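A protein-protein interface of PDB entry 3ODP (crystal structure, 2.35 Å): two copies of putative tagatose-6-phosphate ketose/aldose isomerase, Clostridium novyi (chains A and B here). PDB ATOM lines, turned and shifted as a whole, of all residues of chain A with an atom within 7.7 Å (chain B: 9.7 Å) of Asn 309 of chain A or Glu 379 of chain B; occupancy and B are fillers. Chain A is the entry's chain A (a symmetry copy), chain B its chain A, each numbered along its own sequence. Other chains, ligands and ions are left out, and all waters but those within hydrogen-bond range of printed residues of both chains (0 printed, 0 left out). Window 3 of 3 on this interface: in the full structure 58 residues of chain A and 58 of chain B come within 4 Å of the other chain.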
ATOM      1  N   ARG A 271      22.739  15.423  19.526  1.00  0.00           N
ATOM      2  CA  ARG A 271      21.832  14.296  19.345  1.00  0.00           C
ATOM      3  C   ARG A 271      20.668  14.611  18.401  1.00  0.00           C
ATOM      4  O   ARG A 271      20.257  13.760  17.620  1.00  0.00           O
ATOM      5  CB  ARG A 271      21.276  13.818  20.694  1.00  0.00           C
ATOM      6  CG  ARG A 271      22.230  12.966  21.510  1.00  0.00           C
ATOM      7  CD  ARG A 271      21.525  12.242  22.650  1.00  0.00           C
ATOM      8  NE  ARG A 271      22.455  11.888  23.725  1.00  0.00           N
ATOM      9  CZ  ARG A 271      22.835  12.711  24.706  1.00  0.00           C
ATOM     10  NH1 ARG A 271      22.352  13.953  24.775  1.00  0.00           N
ATOM     11  NH2 ARG A 271      23.707  12.291  25.631  1.00  0.00           N
ATOM     12  N   LYS A 275      24.174  15.223  14.560  1.00  0.00           N
ATOM     13  CA  LYS A 275      24.830  13.917  14.682  1.00  0.00           C
ATOM     14  C   LYS A 275      24.805  13.061  13.408  1.00  0.00           C
ATOM     15  O   LYS A 275      25.713  12.257  13.175  1.00  0.00           O
ATOM     16  CB  LYS A 275      24.118  13.150  15.801  1.00  0.00           C
ATOM     17  CG  LYS A 275      24.719  11.814  16.169  1.00  0.00           C
ATOM     18  CD  LYS A 275      23.817  11.105  17.166  1.00  0.00           C
ATOM     19  CE  LYS A 275      24.283   9.694  17.388  1.00  0.00           C
ATOM     20  NZ  LYS A 275      23.909   9.211  18.741  1.00  0.00           N
ATOM     21  N   SER A 276      23.753  13.204  12.603  1.00  0.00           N
ATOM     22  CA  SER A 276      23.660  12.494  11.318  1.00  0.00           C
ATOM     23  C   SER A 276      24.986  12.534  10.552  1.00  0.00           C
ATOM     24  O   SER A 276      25.313  11.609   9.827  1.00  0.00           O
ATOM     25  CB  SER A 276      22.556  13.094  10.448  1.00  0.00           C
ATOM     26  OG  SER A 276      21.311  13.080  11.120  1.00  0.00           O
ATOM     27  N   ILE A 278      27.963  11.887  11.394  1.00  0.00           N
ATOM     28  CA  ILE A 278      28.953  10.849  11.725  1.00  0.00           C
ATOM     29  C   ILE A 278      29.023   9.736  10.675  1.00  0.00           C
ATOM     30  O   ILE A 278      28.155   8.864  10.629  1.00  0.00           O
ATOM     31  CB  ILE A 278      28.672  10.180  13.095  1.00  0.00           C
ATOM     32  CG1 ILE A 278      28.761  11.191  14.236  1.00  0.00           C
ATOM     33  CG2 ILE A 278      29.665   9.057  13.361  1.00  0.00           C
ATOM     34  CD1 ILE A 278      28.379  10.607  15.575  1.00  0.00           C
ATOM     35  N   ASP A 279      30.063   9.786   9.842  1.00  0.00           N
ATOM     36  CA  ASP A 279      30.435   8.684   8.961  1.00  0.00           C
ATOM     37  C   ASP A 279      31.751   8.086   9.469  1.00  0.00           C
ATOM     38  O   ASP A 279      32.301   8.548  10.480  1.00  0.00           O
ATOM     39  CB  ASP A 279      30.552   9.156   7.498  1.00  0.00           C
ATOM     40  CG  ASP A 279      31.808  10.010   7.226  1.00  0.00           C
ATOM     41  OD1 ASP A 279      32.713  10.115   8.083  1.00  0.00           O
ATOM     42  OD2 ASP A 279      31.893  10.579   6.120  1.00  0.00           O
ATOM     43  N   ASP A 280      32.265   7.095   8.740  1.00  0.00           N
ATOM     44  CA  ASP A 280      33.468   6.346   9.135  1.00  0.00           C
ATOM     45  C   ASP A 280      34.776   7.123   8.943  1.00  0.00           C
ATOM     46  O   ASP A 280      35.839   6.674   9.382  1.00  0.00           O
ATOM     47  CB  ASP A 280      33.555   5.035   8.343  1.00  0.00           C
ATOM     48  CG  ASP A 280      32.301   4.186   8.466  1.00  0.00           C
ATOM     49  OD1 ASP A 280      31.200   4.754   8.636  1.00  0.00           O
ATOM     50  OD2 ASP A 280      32.416   2.943   8.374  1.00  0.00           O
ATOM     51  N   GLU A 304      28.080   7.421  24.137  1.00  0.00           N
ATOM     52  CA  GLU A 304      27.135   7.147  23.064  1.00  0.00           C
ATOM     53  C   GLU A 304      27.789   7.182  21.683  1.00  0.00           C
ATOM     54  O   GLU A 304      27.560   6.293  20.869  1.00  0.00           O
ATOM     55  CB  GLU A 304      26.002   8.159  23.135  1.00  0.00           C
ATOM     56  CG  GLU A 304      25.270   8.350  21.834  1.00  0.00           C
ATOM     57  CD  GLU A 304      23.947   9.030  22.032  1.00  0.00           C
ATOM     58  OE1 GLU A 304      23.235   8.658  22.985  1.00  0.00           O
ATOM     59  OE2 GLU A 304      23.631   9.935  21.241  1.00  0.00           O
ATOM     60  N   VAL A 305      28.574   8.223  21.409  1.00  0.00           N
ATOM     61  CA  VAL A 305      29.208   8.355  20.098  1.00  0.00           C
ATOM     62  C   VAL A 305      30.363   7.350  19.913  1.00  0.00           C
ATOM     63  O   VAL A 305      30.636   6.906  18.793  1.00  0.00           O
ATOM     64  CB  VAL A 305      29.682   9.802  19.830  1.00  0.00           C
ATOM     65  CG1 VAL A 305      30.666  10.262  20.907  1.00  0.00           C
ATOM     66  CG2 VAL A 305      30.322   9.909  18.439  1.00  0.00           C
ATOM     67  N   TYR A 306      31.026   6.983  21.009  1.00  0.00           N
ATOM     68  CA  TYR A 306      32.133   6.020  20.957  1.00  0.00           C
ATOM     69  C   TYR A 306      31.599   4.590  20.694  1.00  0.00           C
ATOM     70  O   TYR A 306      32.249   3.780  20.040  1.00  0.00           O
ATOM     71  CB  TYR A 306      32.961   6.120  22.249  1.00  0.00           C
ATOM     72  CG  TYR A 306      34.123   5.149  22.344  1.00  0.00           C
ATOM     73  CD1 TYR A 306      35.119   5.119  21.372  1.00  0.00           C
ATOM     74  CD2 TYR A 306      34.229   4.269  23.416  1.00  0.00           C
ATOM     75  CE1 TYR A 306      36.184   4.223  21.461  1.00  0.00           C
ATOM     76  CE2 TYR A 306      35.286   3.369  23.511  1.00  0.00           C
ATOM     77  CZ  TYR A 306      36.261   3.347  22.534  1.00  0.00           C
ATOM     78  OH  TYR A 306      37.307   2.453  22.631  1.00  0.00           O
ATOM     79  N   SER A 307      30.385   4.330  21.170  1.00  0.00           N
ATOM     80  CA  SER A 307      29.703   3.055  20.985  1.00  0.00           C
ATOM     81  C   SER A 307      29.161   2.778  19.569  1.00  0.00           C
ATOM     82  O   SER A 307      29.198   1.637  19.124  1.00  0.00           O
ATOM     83  CB  SER A 307      28.529   2.960  21.968  1.00  0.00           C
ATOM     84  OG  SER A 307      28.975   3.071  23.306  1.00  0.00           O
ATOM     85  N   GLN A 308      28.681   3.804  18.867  1.00  0.00           N
ATOM     86  CA  GLN A 308      27.743   3.601  17.737  1.00  0.00           C
ATOM     87  C   GLN A 308      28.305   3.067  16.391  1.00  0.00           C
ATOM     88  O   GLN A 308      28.178   3.716  15.357  1.00  0.00           O
ATOM     89  CB  GLN A 308      26.908   4.883  17.507  1.00  0.00           C
ATOM     90  CG  GLN A 308      27.518   5.962  16.590  1.00  0.00           C
ATOM     91  CD  GLN A 308      26.749   7.269  16.650  1.00  0.00           C
ATOM     92  OE1 GLN A 308      26.554   7.823  17.727  1.00  0.00           O
ATOM     93  NE2 GLN A 308      26.305   7.765  15.496  1.00  0.00           N
ATOM     94  N   ASN A 309      28.866   1.863  16.387  1.00  0.00           N
ATOM     95  CA  ASN A 309      29.358   1.250  15.141  1.00  0.00           C
ATOM     96  C   ASN A 309      30.269   2.185  14.350  1.00  0.00           C
ATOM     97  O   ASN A 309      30.666   3.233  14.847  1.00  0.00           O
ATOM     98  CB  ASN A 309      28.179   0.820  14.258  1.00  0.00           C
ATOM     99  CG  ASN A 309      27.446  -0.356  14.815  1.00  0.00           C
ATOM    100  OD1 ASN A 309      26.228  -0.325  14.970  1.00  0.00           O
ATOM    101  ND2 ASN A 309      28.180  -1.419  15.118  1.00  0.00           N
ATOM    102  N   GLY A 310      30.635   1.790  13.135  1.00  0.00           N
ATOM    103  CA  GLY A 310      31.248   2.718  12.191  1.00  0.00           C
ATOM    104  C   GLY A 310      32.739   2.937  12.338  1.00  0.00           C
ATOM    105  O   GLY A 310      33.352   3.553  11.467  1.00  0.00           O
ATOM    106  N   ASN A 311      33.330   2.473  13.439  1.00  0.00           N
ATOM    107  CA  ASN A 311      34.781   2.518  13.613  1.00  0.00           C
ATOM    108  C   ASN A 311      35.368   3.942  13.602  1.00  0.00           C
ATOM    109  O   ASN A 311      36.535   4.131  13.943  1.00  0.00           O
ATOM    110  CB  ASN A 311      35.466   1.636  12.557  1.00  0.00           C
ATOM    111  N   HIS A 312      34.552   4.929  13.220  1.00  0.00           N
ATOM    112  CA  HIS A 312      34.898   6.358  13.314  1.00  0.00           C
ATOM    113  C   HIS A 312      35.445   6.691  14.692  1.00  0.00           C
ATOM    114  O   HIS A 312      35.216   5.942  15.649  1.00  0.00           O
ATOM    115  CB  HIS A 312      33.655   7.214  13.073  1.00  0.00           C
ATOM    116  CG  HIS A 312      32.577   6.984  14.082  1.00  0.00           C
ATOM    117  ND1 HIS A 312      31.590   6.034  13.916  1.00  0.00           N
ATOM    118  CD2 HIS A 312      32.370   7.537  15.297  1.00  0.00           C
ATOM    119  CE1 HIS A 312      30.808   6.034  14.979  1.00  0.00           C
ATOM    120  NE2 HIS A 312      31.262   6.935  15.832  1.00  0.00           N
ATOM    121  N   LYS A 313      36.126   7.833  14.800  1.00  0.00           N
ATOM    122  CA  LYS A 313      36.999   8.083  15.939  1.00  0.00           C
ATOM    123  C   LYS A 313      36.629   9.339  16.716  1.00  0.00           C
ATOM    124  O   LYS A 313      36.201  10.350  16.147  1.00  0.00           O
ATOM    125  CB  LYS A 313      38.457   8.138  15.467  1.00  0.00           C
ATOM    126  N   PHE B 175      10.186  11.562  10.554  1.00  0.00           N
ATOM    127  CA  PHE B 175      11.400  11.858  11.293  1.00  0.00           C
ATOM    128  C   PHE B 175      11.571  13.378  11.381  1.00  0.00           C
ATOM    129  O   PHE B 175      11.628  13.955  12.463  1.00  0.00           O
ATOM    130  CB  PHE B 175      12.590  11.195  10.588  1.00  0.00           C
ATOM    131  CG  PHE B 175      13.926  11.364  11.296  1.00  0.00           C
ATOM    132  CD1 PHE B 175      14.689  12.506  11.112  1.00  0.00           C
ATOM    133  CD2 PHE B 175      14.445  10.340  12.084  1.00  0.00           C
ATOM    134  CE1 PHE B 175      15.951  12.651  11.748  1.00  0.00           C
ATOM    135  CE2 PHE B 175      15.686  10.470  12.714  1.00  0.00           C
ATOM    136  CZ  PHE B 175      16.439  11.631  12.547  1.00  0.00           C
ATOM    137  N   ALA B 257      20.870  10.987   5.974  1.00  0.00           N
ATOM    138  CA  ALA B 257      21.595  10.131   6.919  1.00  0.00           C
ATOM    139  C   ALA B 257      23.079  10.481   6.930  1.00  0.00           C
ATOM    140  O   ALA B 257      23.931   9.604   7.042  1.00  0.00           O
ATOM    141  CB  ALA B 257      21.392   8.653   6.573  1.00  0.00           C
ATOM    142  N   GLY B 258      23.366  11.775   6.811  1.00  0.00           N
ATOM    143  CA  GLY B 258      24.729  12.281   6.737  1.00  0.00           C
ATOM    144  C   GLY B 258      25.494  11.785   5.524  1.00  0.00           C
ATOM    145  O   GLY B 258      26.677  11.436   5.632  1.00  0.00           O
ATOM    146  N   ASN B 373      12.013   7.638   8.002  1.00  0.00           N
ATOM    147  CA  ASN B 373      12.987   7.178   8.993  1.00  0.00           C
ATOM    148  C   ASN B 373      14.343   6.982   8.319  1.00  0.00           C
ATOM    149  O   ASN B 373      14.705   5.856   7.965  1.00  0.00           O
ATOM    150  CB  ASN B 373      12.528   5.854   9.608  1.00  0.00           C
ATOM    151  CG  ASN B 373      11.224   5.989  10.385  1.00  0.00           C
ATOM    152  OD1 ASN B 373      11.066   6.920  11.181  1.00  0.00           O
ATOM    153  ND2 ASN B 373      10.279   5.060  10.155  1.00  0.00           N
ATOM    154  N   PRO B 374      15.085   8.078   8.108  1.00  0.00           N
ATOM    155  CA  PRO B 374      16.348   8.025   7.368  1.00  0.00           C
ATOM    156  C   PRO B 374      17.455   7.326   8.144  1.00  0.00           C
ATOM    157  O   PRO B 374      18.464   6.929   7.554  1.00  0.00           O
ATOM    158  CB  PRO B 374      16.693   9.500   7.167  1.00  0.00           C
ATOM    159  CG  PRO B 374      16.130  10.163   8.349  1.00  0.00           C
ATOM    160  CD  PRO B 374      14.852   9.414   8.676  1.00  0.00           C
ATOM    161  N   CYS B 375      17.257   7.174   9.451  1.00  0.00           N
ATOM    162  CA  CYS B 375      18.131   6.369  10.286  1.00  0.00           C
ATOM    163  C   CYS B 375      17.344   5.220  10.922  1.00  0.00           C
ATOM    164  O   CYS B 375      17.067   5.236  12.122  1.00  0.00           O
ATOM    165  CB  CYS B 375      18.778   7.257  11.352  1.00  0.00           C
ATOM    166  SG  CYS B 375      20.266   6.544  12.087  1.00  0.00           S
ATOM    167  N   PRO B 376      16.971   4.211  10.113  1.00  0.00           N
ATOM    168  CA  PRO B 376      16.270   3.070  10.695  1.00  0.00           C
ATOM    169  C   PRO B 376      17.116   2.377  11.761  1.00  0.00           C
ATOM    170  O   PRO B 376      16.583   1.940  12.777  1.00  0.00           O
ATOM    171  CB  PRO B 376      16.037   2.141   9.496  1.00  0.00           C
ATOM    172  CG  PRO B 376      16.234   2.980   8.293  1.00  0.00           C
ATOM    173  CD  PRO B 376      17.242   4.003   8.681  1.00  0.00           C
ATOM    174  N   THR B 377      18.427   2.310  11.536  1.00  0.00           N
ATOM    175  CA  THR B 377      19.358   1.733  12.508  1.00  0.00           C
ATOM    176  C   THR B 377      19.414   2.507  13.831  1.00  0.00           C
ATOM    177  O   THR B 377      20.049   2.065  14.784  1.00  0.00           O
ATOM    178  CB  THR B 377      20.778   1.616  11.919  1.00  0.00           C
ATOM    179  OG1 THR B 377      21.073   2.783  11.142  1.00  0.00           O
ATOM    180  CG2 THR B 377      20.883   0.376  11.031  1.00  0.00           C
ATOM    181  N   GLY B 378      18.771   3.668  13.883  1.00  0.00           N
ATOM    182  CA  GLY B 378      18.501   4.341  15.149  1.00  0.00           C
ATOM    183  C   GLY B 378      19.639   5.121  15.794  1.00  0.00           C
ATOM    184  O   GLY B 378      19.558   5.450  16.976  1.00  0.00           O
ATOM    185  N   GLU B 379      20.698   5.432  15.049  1.00  0.00           N
ATOM    186  CA  GLU B 379      21.770   6.281  15.598  1.00  0.00           C
ATOM    187  C   GLU B 379      21.188   7.651  16.006  1.00  0.00           C
ATOM    188  O   GLU B 379      21.471   8.156  17.098  1.00  0.00           O
ATOM    189  CB  GLU B 379      22.942   6.425  14.612  1.00  0.00           C
ATOM    190  CG  GLU B 379      24.000   5.301  14.701  1.00  0.00           C
ATOM    191  CD  GLU B 379      23.492   3.919  14.289  1.00  0.00           C
ATOM    192  OE1 GLU B 379      22.401   3.828  13.683  1.00  0.00           O
ATOM    193  OE2 GLU B 379      24.193   2.919  14.576  1.00  0.00           O
ATOM    194  N   VAL B 380      20.367   8.231  15.127  1.00  0.00           N
ATOM    195  CA  VAL B 380      19.526   9.381  15.465  1.00  0.00           C
ATOM    196  C   VAL B 380      18.053   8.949  15.406  1.00  0.00           C
ATOM    197  O   VAL B 380      17.705   8.002  14.701  1.00  0.00           O
ATOM    198  CB  VAL B 380      19.759  10.568  14.511  1.00  0.00           C
ATOM    199  CG1 VAL B 380      19.462  11.881  15.218  1.00  0.00           C
ATOM    200  CG2 VAL B 380      21.177  10.573  14.013  1.00  0.00           C
ATOM    201  N   ASN B 381      17.191   9.637  16.145  1.00  0.00           N
ATOM    202  CA  ASN B 381      15.784   9.241  16.258  1.00  0.00           C
ATOM    203  C   ASN B 381      14.814  10.411  16.083  1.00  0.00           C
ATOM    204  O   ASN B 381      15.222  11.567  16.093  1.00  0.00           O
ATOM    205  CB  ASN B 381      15.545   8.568  17.616  1.00  0.00           C
ATOM    206  CG  ASN B 381      16.141   7.177  17.695  1.00  0.00           C
ATOM    207  OD1 ASN B 381      15.587   6.211  17.150  1.00  0.00           O
ATOM    208  ND2 ASN B 381      17.261   7.058  18.396  1.00  0.00           N
ATOM    209  N   ARG B 382      13.526  10.094  15.905  1.00  0.00           N
ATOM    210  CA  ARG B 382      12.458  11.104  15.905  1.00  0.00           C
ATOM    211  C   ARG B 382      12.302  11.714  17.298  1.00  0.00           C
ATOM    212  O   ARG B 382      12.218  12.927  17.438  1.00  0.00           O
ATOM    213  CB  ARG B 382      11.123  10.511  15.447  1.00  0.00           C
ATOM    214  CG  ARG B 382       9.978  11.529  15.423  1.00  0.00           C
ATOM    215  CD  ARG B 382       8.677  10.934  14.913  1.00  0.00           C
ATOM    216  NE  ARG B 382       7.512  11.685  15.394  1.00  0.00           N
ATOM    217  CZ  ARG B 382       6.899  11.486  16.562  1.00  0.00           C
ATOM    218  NH1 ARG B 382       7.327  10.551  17.415  1.00  0.00           N
ATOM    219  NH2 ARG B 382       5.847  12.235  16.887  1.00  0.00           N
ATOM    220  N   VAL B 383      12.235  10.864  18.316  1.00  0.00           N
ATOM    221  CA  VAL B 383      12.270  11.309  19.710  1.00  0.00           C
ATOM    222  C   VAL B 383      13.640  10.930  20.256  1.00  0.00           C
ATOM    223  O   VAL B 383      14.100   9.816  20.036  1.00  0.00           O
ATOM    224  CB  VAL B 383      11.165  10.638  20.534  1.00  0.00           C
ATOM    225  CG1 VAL B 383      11.241  11.069  21.994  1.00  0.00           C
ATOM    226  CG2 VAL B 383       9.807  10.954  19.931  1.00  0.00           C
ATOM    227  N   VAL B 384      14.292  11.848  20.963  1.00  0.00           N
ATOM    228  CA  VAL B 384      15.702  11.664  21.320  1.00  0.00           C
ATOM    229  C   VAL B 384      15.896  10.546  22.353  1.00  0.00           C
ATOM    230  O   VAL B 384      15.238  10.512  23.390  1.00  0.00           O
ATOM    231  CB  VAL B 384      16.357  12.992  21.790  1.00  0.00           C
ATOM    232  CG1 VAL B 384      15.711  13.515  23.065  1.00  0.00           C
ATOM    233  CG2 VAL B 384      17.855  12.803  21.989  1.00  0.00           C
ATOM    234  N   LYS B 385      16.804   9.625  22.040  1.00  0.00           N
ATOM    235  CA  LYS B 385      17.033   8.450  22.872  1.00  0.00           C
ATOM    236  C   LYS B 385      18.392   8.564  23.524  1.00  0.00           C
ATOM    237  O   LYS B 385      19.321   9.164  22.969  1.00  0.00           O
ATOM    238  CB  LYS B 385      16.942   7.163  22.043  1.00  0.00           C
ATOM    239  N   GLY B 386      18.493   7.999  24.722  1.00  0.00           N
ATOM    240  CA  GLY B 386      19.722   8.040  25.496  1.00  0.00           C
ATOM    241  C   GLY B 386      20.065   9.385  26.112  1.00  0.00           C
ATOM    242  O   GLY B 386      21.239   9.655  26.351  1.00  0.00           O
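The backbone carbonyl oxygen of Glu 379 of chain B sits at hydrogen-bond distance from the side-chain amino group of Lys 275 of chain A.
NE of Arg 271 of chain A lies within salt-bridge range of OE2 of Glu 304 of chain A (3.4 Å).
The side-chain amino group (NZ) of Lys 275 of chain A sits close to the side-chain amide oxygen (OE1) of Gln 308 of chain A.
The side-chain carboxylate (OE2) of Glu 304 of chain A is in salt-bridge range of the side-chain amino group (NZ) of Lys 275 of chain A (2.6 Å).
The side-chain sulfur (SG) of Cys 375 of chain B is in hydrogen-bond range of the backbone NH (N) of Val 380 of chain B (3.5 Å).
The side-chain sulfur (SG) of Cys 375 of chain B is in hydrogen-bond range of the backbone NH (N) of Glu 379 of chain B (3.2 Å).
A ring nitrogen (ND1) of His 312 of chain A lies close to the backbone carbonyl oxygen of Asn 309 of chain A, at 3.1 Å.
Arg 271 of chain A touches Val 380 of chain B (O to CG1, 3.2 Å).
Val 384 of chain B touches Arg 271 of chain A.
Arg 271 of chain A touches Lys 385 of chain B (CD to O, 3.8 Å).
NE of Arg 271 of chain A touches O of Gly 386 of chain B, at 3.7 Å.
O of Ser 276 of chain A touches O of Ala 257 of chain B, 3.7 Å away.
O of Ser 276 of chain A touches CA of Gly 258 of chain B, at 3.2 Å.
OG of Ser 276 of chain A touches CG2 of Val 380 of chain B, at 3.8 Å.
Glu 304 of chain A touches Lys 385 of chain B.
Glu 379 of chain B touches Gln 308 of chain A (CG to NE2, 3.5 Å).
Asn 309 of chain A touches Glu 379 of chain B.
Of chain B, only Glu 379 (3.8 Å) comes within 4 Å of Asn 309 of chain A.
Glu 379 of chain B touches three residues of chain A.
Gln 308 of chain A touches just one residue of chain B: Glu 379 (3.5 Å).
No residue of chain A comes within 4 Å of Gly 378 of chain B.
Of the printed residues of chain A, Val 380 of chain B touches Arg 271 and Ser 276.
Of the printed residues of chain B, Lys 275 of chain A touches Glu 379 (3.1 Å).
Printed residues of chain A within 4 Å of Ala 257 of chain B: Ser 276 (3.7 Å).
Of the printed residues of chain A, Gly 386 of chain B touches Arg 271.
Phe 175 of chain B touches none of the printed residues of chain A.
The nearest residue of chain B that does not touch Asn 309 of chain A is Thr 377 of chain B (6.5 Å).
The nearest residue of chain A that does not touch Glu 379 of chain B is Glu 304 of chain A (5.0 Å).
Of the 16 printed residues of chain A, 6 touch a printed residue of chain B.
Printed residues of chain B that touch a printed residue of chain A: Ala 257, Gly 258, Glu 379, Val 380, Val 384, Lys 385 and Gly 386.
Hydrophobic or aromatic side chains of chain B that line the printed part of chain A: Val 380 and Val 384.
Among the printed residues, 11 pairs touch across the chains.
Among the printed residues, no Asp or Glu carboxylate lies within 4 Å of a Lys or Arg side-chain nitrogen of the other chain.
No position is printed for both chains.
Of the 11 pairs that touch across the chains among the printed residues, none has its exchanged pair printed and touching as well.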
